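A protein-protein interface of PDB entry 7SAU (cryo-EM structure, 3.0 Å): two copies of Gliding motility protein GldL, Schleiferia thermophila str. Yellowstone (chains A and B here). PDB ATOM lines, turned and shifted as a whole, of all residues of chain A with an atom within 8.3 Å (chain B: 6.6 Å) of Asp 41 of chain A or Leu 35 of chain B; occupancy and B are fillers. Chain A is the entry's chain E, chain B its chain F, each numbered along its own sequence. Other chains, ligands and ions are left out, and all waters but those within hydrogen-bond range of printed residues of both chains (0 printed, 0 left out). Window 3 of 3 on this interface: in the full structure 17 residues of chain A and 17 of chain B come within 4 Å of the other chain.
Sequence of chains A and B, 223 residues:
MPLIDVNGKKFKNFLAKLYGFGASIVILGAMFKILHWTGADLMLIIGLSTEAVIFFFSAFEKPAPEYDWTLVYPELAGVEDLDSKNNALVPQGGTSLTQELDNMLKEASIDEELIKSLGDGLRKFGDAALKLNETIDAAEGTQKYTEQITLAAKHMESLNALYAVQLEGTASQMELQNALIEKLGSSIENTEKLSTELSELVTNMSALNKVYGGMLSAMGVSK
Of the 18 printed residues of chain A, 4 touch a printed residue of chain B. Printed residues of chain A that touch a printed residue of chain B: Asp 41, Leu 44, Ile 45 and Leu 48. Hydrophobic or aromatic side chains of chain A within 4 Å of the printed part of chain B: Leu 44, Ile 45 and Leu 48. Of the 8 printed residues of chain B, 4 touch a printed residue of chain A. Among the printed residues, 8 pairs touch across the chains. Among the printed residues, no Asp or Glu carboxylate lies within 4 Å of a Lys or Arg side-chain nitrogen of the other chain.
Asp 41 of chain A touches Ile 34 of chain B. OD2 of Asp 41 of chain A touches CD1 of Leu 35 of chain B, 3.6 Å away. CG2 of Ile 34 of chain B touches CD1 of Leu 44 of chain A, 3.98 Å away. Ile 45 of chain A touches Leu 35 of chain B (CG1 to CD2, 3.6 Å). CD1 of Ile 45 of chain A touches CH2 of Trp 37 of chain B (3.7 Å). CD1 of Leu 48 of chain A touches CB of Met 31 of chain B, 3.9 Å away. Ile 34 of chain B touches Leu 48 of chain A (CD1 to CD1, 3.8 Å).
Leu 35 of chain B touches two residues of chain A. Of the printed residues of chain A, Met 31 of chain B touches Ile 45 and Leu 48. Of the printed residues of chain A, Trp 37 of chain B touches Ile 45. Of the printed residues of chain B, Leu 48 of chain A touches Met 31 (3.9 Å) and Ile 34 (3.8 Å). Lys 33 of chain B touches none of the printed residues of chain A. Gly 39 of chain A touches none of the printed residues of chain B. The nearest residue of chain B that does not touch Asp 41 of chain A is His 36 of chain B (6.2 Å). The nearest printed residue of chain B that does not touch Leu 48 of chain A is Ala 30 of chain B (4.6 Å).
The side-chain sulfur of Met 31 of chain B sits close to the backbone carbonyl oxygen of Ile 45 of chain A, 3.5 Å away.
4 positions are printed for both chains. Of the 8 pairs that touch across the chains among the printed residues, none has its exchanged pair printed and touching as well.
The backbone carbonyl oxygen of Phe 32 of chain B lies within hydrogen-bond range of the backbone NH of Trp 37 of chain B. OD1 of Asp 41 of chain A lies within salt-bridge range of NZ of Lys 33 of chain A (3.7 Å).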
ATOM      1  N   ILE A  25       4.853  11.195  19.418  1.00  0.00           N
ATOM      2  CA  ILE A  25       5.030  12.297  20.358  1.00  0.00           C
ATOM      3  C   ILE A  25       3.842  13.249  20.302  1.00  0.00           C
ATOM      4  O   ILE A  25       3.429  13.804  21.326  1.00  0.00           O
ATOM      5  CB  ILE A  25       6.357  13.026  20.091  1.00  0.00           C
ATOM      6  CG1 ILE A  25       7.482  12.025  19.846  1.00  0.00           C
ATOM      7  CG2 ILE A  25       6.723  13.894  21.269  1.00  0.00           C
ATOM      8  CD1 ILE A  25       7.819  11.182  21.046  1.00  0.00           C
ATOM      9  N   LEU A  28       0.981  11.590  22.267  1.00  0.00           N
ATOM     10  CA  LEU A  28       1.188  11.680  23.707  1.00  0.00           C
ATOM     11  C   LEU A  28       1.164  13.125  24.179  1.00  0.00           C
ATOM     12  O   LEU A  28       0.634  13.421  25.254  1.00  0.00           O
ATOM     13  CB  LEU A  28       2.505  11.013  24.086  1.00  0.00           C
ATOM     14  CG  LEU A  28       2.578   9.512  23.826  1.00  0.00           C
ATOM     15  CD1 LEU A  28       3.901   8.960  24.311  1.00  0.00           C
ATOM     16  CD2 LEU A  28       1.418   8.810  24.498  1.00  0.00           C
ATOM     17  N   GLY A  29       1.733  14.037  23.392  1.00  0.00           N
ATOM     18  CA  GLY A  29       1.698  15.440  23.756  1.00  0.00           C
ATOM     19  C   GLY A  29       0.291  15.989  23.864  1.00  0.00           C
ATOM     20  O   GLY A  29       0.020  16.847  24.704  1.00  0.00           O
ATOM     21  N   ALA A  30      -0.621  15.509  23.017  1.00  0.00           N
ATOM     22  CA  ALA A  30      -2.017  15.910  23.135  1.00  0.00           C
ATOM     23  C   ALA A  30      -2.667  15.286  24.360  1.00  0.00           C
ATOM     24  O   ALA A  30      -3.502  15.917  25.014  1.00  0.00           O
ATOM     25  CB  ALA A  30      -2.783  15.528  21.874  1.00  0.00           C
ATOM     26  N   PHE A  32      -1.126  14.538  27.177  1.00  0.00           N
ATOM     27  CA  PHE A  32      -0.653  15.342  28.296  1.00  0.00           C
ATOM     28  C   PHE A  32      -1.349  16.695  28.327  1.00  0.00           C
ATOM     29  O   PHE A  32      -1.711  17.190  29.398  1.00  0.00           O
ATOM     30  CB  PHE A  32       0.861  15.521  28.209  1.00  0.00           C
ATOM     31  CG  PHE A  32       1.647  14.338  28.701  1.00  0.00           C
ATOM     32  CD1 PHE A  32       1.279  13.050  28.365  1.00  0.00           C
ATOM     33  CD2 PHE A  32       2.761  14.520  29.493  1.00  0.00           C
ATOM     34  CE1 PHE A  32       2.000  11.970  28.811  1.00  0.00           C
ATOM     35  CE2 PHE A  32       3.487  13.441  29.943  1.00  0.00           C
ATOM     36  CZ  PHE A  32       3.105  12.165  29.601  1.00  0.00           C
ATOM     37  N   LYS A  33      -1.544  17.304  27.156  1.00  0.00           N
ATOM     38  CA  LYS A  33      -2.142  18.633  27.076  1.00  0.00           C
ATOM     39  C   LYS A  33      -3.595  18.629  27.532  1.00  0.00           C
ATOM     40  O   LYS A  33      -4.025  19.535  28.253  1.00  0.00           O
ATOM     41  CB  LYS A  33      -2.029  19.159  25.647  1.00  0.00           C
ATOM     42  CG  LYS A  33      -2.591  20.544  25.429  1.00  0.00           C
ATOM     43  CD  LYS A  33      -1.756  21.601  26.113  1.00  0.00           C
ATOM     44  CE  LYS A  33      -2.277  22.985  25.792  1.00  0.00           C
ATOM     45  NZ  LYS A  33      -1.516  24.042  26.507  1.00  0.00           N
ATOM     46  N   TRP A  37      -0.931  17.718  32.192  1.00  0.00           N
ATOM     47  CA  TRP A  37       0.271  17.139  32.766  1.00  0.00           C
ATOM     48  C   TRP A  37       1.480  17.981  32.377  1.00  0.00           C
ATOM     49  O   TRP A  37       1.480  18.672  31.357  1.00  0.00           O
ATOM     50  CB  TRP A  37       0.438  15.691  32.308  1.00  0.00           C
ATOM     51  CG  TRP A  37      -0.612  14.791  32.868  1.00  0.00           C
ATOM     52  CD1 TRP A  37      -1.567  15.124  33.775  1.00  0.00           C
ATOM     53  CD2 TRP A  37      -0.822  13.411  32.556  1.00  0.00           C
ATOM     54  NE1 TRP A  37      -2.359  14.040  34.052  1.00  0.00           N
ATOM     55  CE2 TRP A  37      -1.921  12.974  33.315  1.00  0.00           C
ATOM     56  CE3 TRP A  37      -0.186  12.501  31.708  1.00  0.00           C
ATOM     57  CZ2 TRP A  37      -2.396  11.672  33.254  1.00  0.00           C
ATOM     58  CZ3 TRP A  37      -0.661  11.211  31.649  1.00  0.00           C
ATOM     59  CH2 TRP A  37      -1.753  10.807  32.416  1.00  0.00           C
ATOM     60  N   THR A  38       2.517  17.917  33.214  1.00  0.00           N
ATOM     61  CA  THR A  38       3.571  18.930  33.175  1.00  0.00           C
ATOM     62  C   THR A  38       4.370  18.885  31.879  1.00  0.00           C
ATOM     63  O   THR A  38       4.859  19.921  31.414  1.00  0.00           O
ATOM     64  CB  THR A  38       4.502  18.764  34.373  1.00  0.00           C
ATOM     65  OG1 THR A  38       5.257  17.557  34.229  1.00  0.00           O
ATOM     66  CG2 THR A  38       3.700  18.702  35.657  1.00  0.00           C
ATOM     67  N   GLY A  39       4.520  17.712  31.278  1.00  0.00           N
ATOM     68  CA  GLY A  39       5.372  17.606  30.112  1.00  0.00           C
ATOM     69  C   GLY A  39       4.672  17.906  28.803  1.00  0.00           C
ATOM     70  O   GLY A  39       5.202  17.609  27.731  1.00  0.00           O
ATOM     71  N   ALA A  40       3.486  18.510  28.882  1.00  0.00           N
ATOM     72  CA  ALA A  40       2.622  18.631  27.712  1.00  0.00           C
ATOM     73  C   ALA A  40       3.271  19.458  26.610  1.00  0.00           C
ATOM     74  O   ALA A  40       3.352  19.022  25.458  1.00  0.00           O
ATOM     75  CB  ALA A  40       1.284  19.243  28.120  1.00  0.00           C
ATOM     76  N   ASP A  41       3.744  20.658  26.945  1.00  0.00           N
ATOM     77  CA  ASP A  41       4.223  21.575  25.919  1.00  0.00           C
ATOM     78  C   ASP A  41       5.574  21.170  25.350  1.00  0.00           C
ATOM     79  O   ASP A  41       5.901  21.569  24.229  1.00  0.00           O
ATOM     80  CB  ASP A  41       4.300  22.992  26.479  1.00  0.00           C
ATOM     81  CG  ASP A  41       2.992  23.744  26.341  1.00  0.00           C
ATOM     82  OD1 ASP A  41       1.991  23.125  25.928  1.00  0.00           O
ATOM     83  OD2 ASP A  41       2.961  24.954  26.646  1.00  0.00           O
ATOM     84  N   LEU A  42       6.373  20.400  26.090  1.00  0.00           N
ATOM     85  CA  LEU A  42       7.660  19.968  25.557  1.00  0.00           C
ATOM     86  C   LEU A  42       7.487  18.873  24.513  1.00  0.00           C
ATOM     87  O   LEU A  42       8.153  18.892  23.473  1.00  0.00           O
ATOM     88  CB  LEU A  42       8.569  19.495  26.688  1.00  0.00           C
ATOM     89  CG  LEU A  42       9.922  18.937  26.248  1.00  0.00           C
ATOM     90  CD1 LEU A  42      10.802  20.040  25.697  1.00  0.00           C
ATOM     91  CD2 LEU A  42      10.608  18.227  27.395  1.00  0.00           C
ATOM     92  N   MET A  43       6.602  17.908  24.769  1.00  0.00           N
ATOM     93  CA  MET A  43       6.341  16.876  23.773  1.00  0.00           C
ATOM     94  C   MET A  43       5.636  17.443  22.550  1.00  0.00           C
ATOM     95  O   MET A  43       5.856  16.963  21.433  1.00  0.00           O
ATOM     96  CB  MET A  43       5.512  15.745  24.377  1.00  0.00           C
ATOM     97  CG  MET A  43       5.974  15.298  25.741  1.00  0.00           C
ATOM     98  SD  MET A  43       4.773  14.230  26.545  1.00  0.00           S
ATOM     99  CE  MET A  43       5.187  12.658  25.806  1.00  0.00           C
ATOM    100  N   LEU A  44       4.785  18.451  22.734  1.00  0.00           N
ATOM    101  CA  LEU A  44       4.151  19.087  21.587  1.00  0.00           C
ATOM    102  C   LEU A  44       5.172  19.818  20.728  1.00  0.00           C
ATOM    103  O   LEU A  44       5.045  19.849  19.502  1.00  0.00           O
ATOM    104  CB  LEU A  44       3.056  20.042  22.049  1.00  0.00           C
ATOM    105  CG  LEU A  44       1.730  19.378  22.404  1.00  0.00           C
ATOM    106  CD1 LEU A  44       0.775  20.393  22.986  1.00  0.00           C
ATOM    107  CD2 LEU A  44       1.129  18.703  21.187  1.00  0.00           C
ATOM    108  N   ILE A  45       6.186  20.421  21.349  1.00  0.00           N
ATOM    109  CA  ILE A  45       7.242  21.071  20.578  1.00  0.00           C
ATOM    110  C   ILE A  45       7.989  20.046  19.737  1.00  0.00           C
ATOM    111  O   ILE A  45       8.222  20.249  18.543  1.00  0.00           O
ATOM    112  CB  ILE A  45       8.203  21.834  21.507  1.00  0.00           C
ATOM    113  CG1 ILE A  45       7.592  23.157  21.948  1.00  0.00           C
ATOM    114  CG2 ILE A  45       9.525  22.090  20.810  1.00  0.00           C
ATOM    115  CD1 ILE A  45       8.383  23.843  23.029  1.00  0.00           C
ATOM    116  N   ILE A  46       8.370  18.924  20.346  1.00  0.00           N
ATOM    117  CA  ILE A  46       9.147  17.920  19.625  1.00  0.00           C
ATOM    118  C   ILE A  46       8.297  17.261  18.548  1.00  0.00           C
ATOM    119  O   ILE A  46       8.743  17.077  17.411  1.00  0.00           O
ATOM    120  CB  ILE A  46       9.724  16.882  20.601  1.00  0.00           C
ATOM    121  CG1 ILE A  46      10.631  17.559  21.625  1.00  0.00           C
ATOM    122  CG2 ILE A  46      10.492  15.821  19.845  1.00  0.00           C
ATOM    123  CD1 ILE A  46      10.871  16.732  22.858  1.00  0.00           C
ATOM    124  N   GLY A  47       7.065  16.886  18.891  1.00  0.00           N
ATOM    125  CA  GLY A  47       6.217  16.206  17.928  1.00  0.00           C
ATOM    126  C   GLY A  47       5.803  17.086  16.765  1.00  0.00           C
ATOM    127  O   GLY A  47       5.809  16.647  15.613  1.00  0.00           O
ATOM    128  N   LEU A  48       5.426  18.332  17.045  1.00  0.00           N
ATOM    129  CA  LEU A  48       4.962  19.210  15.977  1.00  0.00           C
ATOM    130  C   LEU A  48       6.122  19.719  15.132  1.00  0.00           C
ATOM    131  O   LEU A  48       5.990  19.853  13.912  1.00  0.00           O
ATOM    132  CB  LEU A  48       4.166  20.375  16.560  1.00  0.00           C
ATOM    133  CG  LEU A  48       2.747  20.049  17.024  1.00  0.00           C
ATOM    134  CD1 LEU A  48       2.089  21.273  17.617  1.00  0.00           C
ATOM    135  CD2 LEU A  48       1.921  19.497  15.882  1.00  0.00           C
ATOM    136  N   ALA B  30       0.850  26.555  14.428  1.00  0.00           N
ATOM    137  CA  ALA B  30       0.067  25.930  15.486  1.00  0.00           C
ATOM    138  C   ALA B  30       0.917  25.669  16.720  1.00  0.00           C
ATOM    139  O   ALA B  30       0.434  25.796  17.849  1.00  0.00           O
ATOM    140  CB  ALA B  30      -0.560  24.632  14.981  1.00  0.00           C
ATOM    141  N   MET B  31       2.184  25.301  16.528  1.00  0.00           N
ATOM    142  CA  MET B  31       3.069  25.081  17.665  1.00  0.00           C
ATOM    143  C   MET B  31       3.385  26.386  18.380  1.00  0.00           C
ATOM    144  O   MET B  31       3.404  26.437  19.613  1.00  0.00           O
ATOM    145  CB  MET B  31       4.362  24.416  17.203  1.00  0.00           C
ATOM    146  CG  MET B  31       5.320  24.101  18.329  1.00  0.00           C
ATOM    147  SD  MET B  31       6.825  23.305  17.760  1.00  0.00           S
ATOM    148  CE  MET B  31       7.624  24.681  16.954  1.00  0.00           C
ATOM    149  N   PHE B  32       3.640  27.453  17.621  1.00  0.00           N
ATOM    150  CA  PHE B  32       3.945  28.742  18.228  1.00  0.00           C
ATOM    151  C   PHE B  32       2.748  29.282  18.993  1.00  0.00           C
ATOM    152  O   PHE B  32       2.903  29.871  20.067  1.00  0.00           O
ATOM    153  CB  PHE B  32       4.384  29.730  17.151  1.00  0.00           C
ATOM    154  CG  PHE B  32       5.851  29.695  16.861  1.00  0.00           C
ATOM    155  CD1 PHE B  32       6.493  28.494  16.630  1.00  0.00           C
ATOM    156  CD2 PHE B  32       6.590  30.859  16.810  1.00  0.00           C
ATOM    157  CE1 PHE B  32       7.837  28.453  16.358  1.00  0.00           C
ATOM    158  CE2 PHE B  32       7.939  30.823  16.539  1.00  0.00           C
ATOM    159  CZ  PHE B  32       8.562  29.617  16.313  1.00  0.00           C
ATOM    160  N   LYS B  33       1.547  29.100  18.447  1.00  0.00           N
ATOM    161  CA  LYS B  33       0.336  29.530  19.134  1.00  0.00           C
ATOM    162  C   LYS B  33       0.119  28.736  20.415  1.00  0.00           C
ATOM    163  O   LYS B  33      -0.320  29.292  21.426  1.00  0.00           O
ATOM    164  CB  LYS B  33      -0.863  29.391  18.199  1.00  0.00           C
ATOM    165  CG  LYS B  33      -2.095  30.149  18.642  1.00  0.00           C
ATOM    166  CD  LYS B  33      -2.049  31.593  18.187  1.00  0.00           C
ATOM    167  CE  LYS B  33      -3.271  32.347  18.670  1.00  0.00           C
ATOM    168  NZ  LYS B  33      -3.230  33.774  18.276  1.00  0.00           N
ATOM    169  N   ILE B  34       0.415  27.435  20.389  1.00  0.00           N
ATOM    170  CA  ILE B  34       0.314  26.614  21.593  1.00  0.00           C
ATOM    171  C   ILE B  34       1.271  27.120  22.663  1.00  0.00           C
ATOM    172  O   ILE B  34       0.910  27.234  23.839  1.00  0.00           O
ATOM    173  CB  ILE B  34       0.573  25.134  21.253  1.00  0.00           C
ATOM    174  CG1 ILE B  34      -0.638  24.519  20.556  1.00  0.00           C
ATOM    175  CG2 ILE B  34       0.900  24.344  22.499  1.00  0.00           C
ATOM    176  CD1 ILE B  34      -0.327  23.280  19.756  1.00  0.00           C
ATOM    177  N   LEU B  35       2.495  27.445  22.270  1.00  0.00           N
ATOM    178  CA  LEU B  35       3.528  27.888  23.192  1.00  0.00           C
ATOM    179  C   LEU B  35       3.467  29.379  23.478  1.00  0.00           C
ATOM    180  O   LEU B  35       4.271  29.871  24.276  1.00  0.00           O
ATOM    181  CB  LEU B  35       4.909  27.528  22.642  1.00  0.00           C
ATOM    182  CG  LEU B  35       5.443  26.130  22.951  1.00  0.00           C
ATOM    183  CD1 LEU B  35       5.608  25.954  24.444  1.00  0.00           C
ATOM    184  CD2 LEU B  35       4.554  25.044  22.382  1.00  0.00           C
ATOM    185  N   HIS B  36       2.540  30.101  22.853  1.00  0.00           N
ATOM    186  CA  HIS B  36       2.399  31.546  23.023  1.00  0.00           C
ATOM    187  C   HIS B  36       3.694  32.277  22.682  1.00  0.00           C
ATOM    188  O   HIS B  36       4.084  33.231  23.353  1.00  0.00           O
ATOM    189  CB  HIS B  36       1.936  31.897  24.438  1.00  0.00           C
ATOM    190  CG  HIS B  36       0.515  31.528  24.716  1.00  0.00           C
ATOM    191  ND1 HIS B  36       0.165  30.411  25.441  1.00  0.00           N
ATOM    192  CD2 HIS B  36      -0.647  32.129  24.369  1.00  0.00           C
ATOM    193  CE1 HIS B  36      -1.150  30.337  25.527  1.00  0.00           C
ATOM    194  NE2 HIS B  36      -1.667  31.368  24.884  1.00  0.00           N
ATOM    195  N   TRP B  37       4.367  31.827  21.628  1.00  0.00           N
ATOM    196  CA  TRP B  37       5.557  32.515  21.163  1.00  0.00           C
ATOM    197  C   TRP B  37       5.172  33.665  20.238  1.00  0.00           C
ATOM    198  O   TRP B  37       4.022  33.797  19.811  1.00  0.00           O
ATOM    199  CB  TRP B  37       6.507  31.542  20.473  1.00  0.00           C
ATOM    200  CG  TRP B  37       7.132  30.585  21.428  1.00  0.00           C
ATOM    201  CD1 TRP B  37       7.161  30.693  22.783  1.00  0.00           C
ATOM    202  CD2 TRP B  37       7.821  29.374  21.108  1.00  0.00           C
ATOM    203  NE1 TRP B  37       7.822  29.626  23.330  1.00  0.00           N
ATOM    204  CE2 TRP B  37       8.238  28.801  22.320  1.00  0.00           C
ATOM    205  CE3 TRP B  37       8.123  28.719  19.914  1.00  0.00           C
ATOM    206  CZ2 TRP B  37       8.940  27.606  22.374  1.00  0.00           C
ATOM    207  CZ3 TRP B  37       8.820  27.533  19.969  1.00  0.00           C
ATOM    208  CH2 TRP B  37       9.222  26.988  21.189  1.00  0.00           C
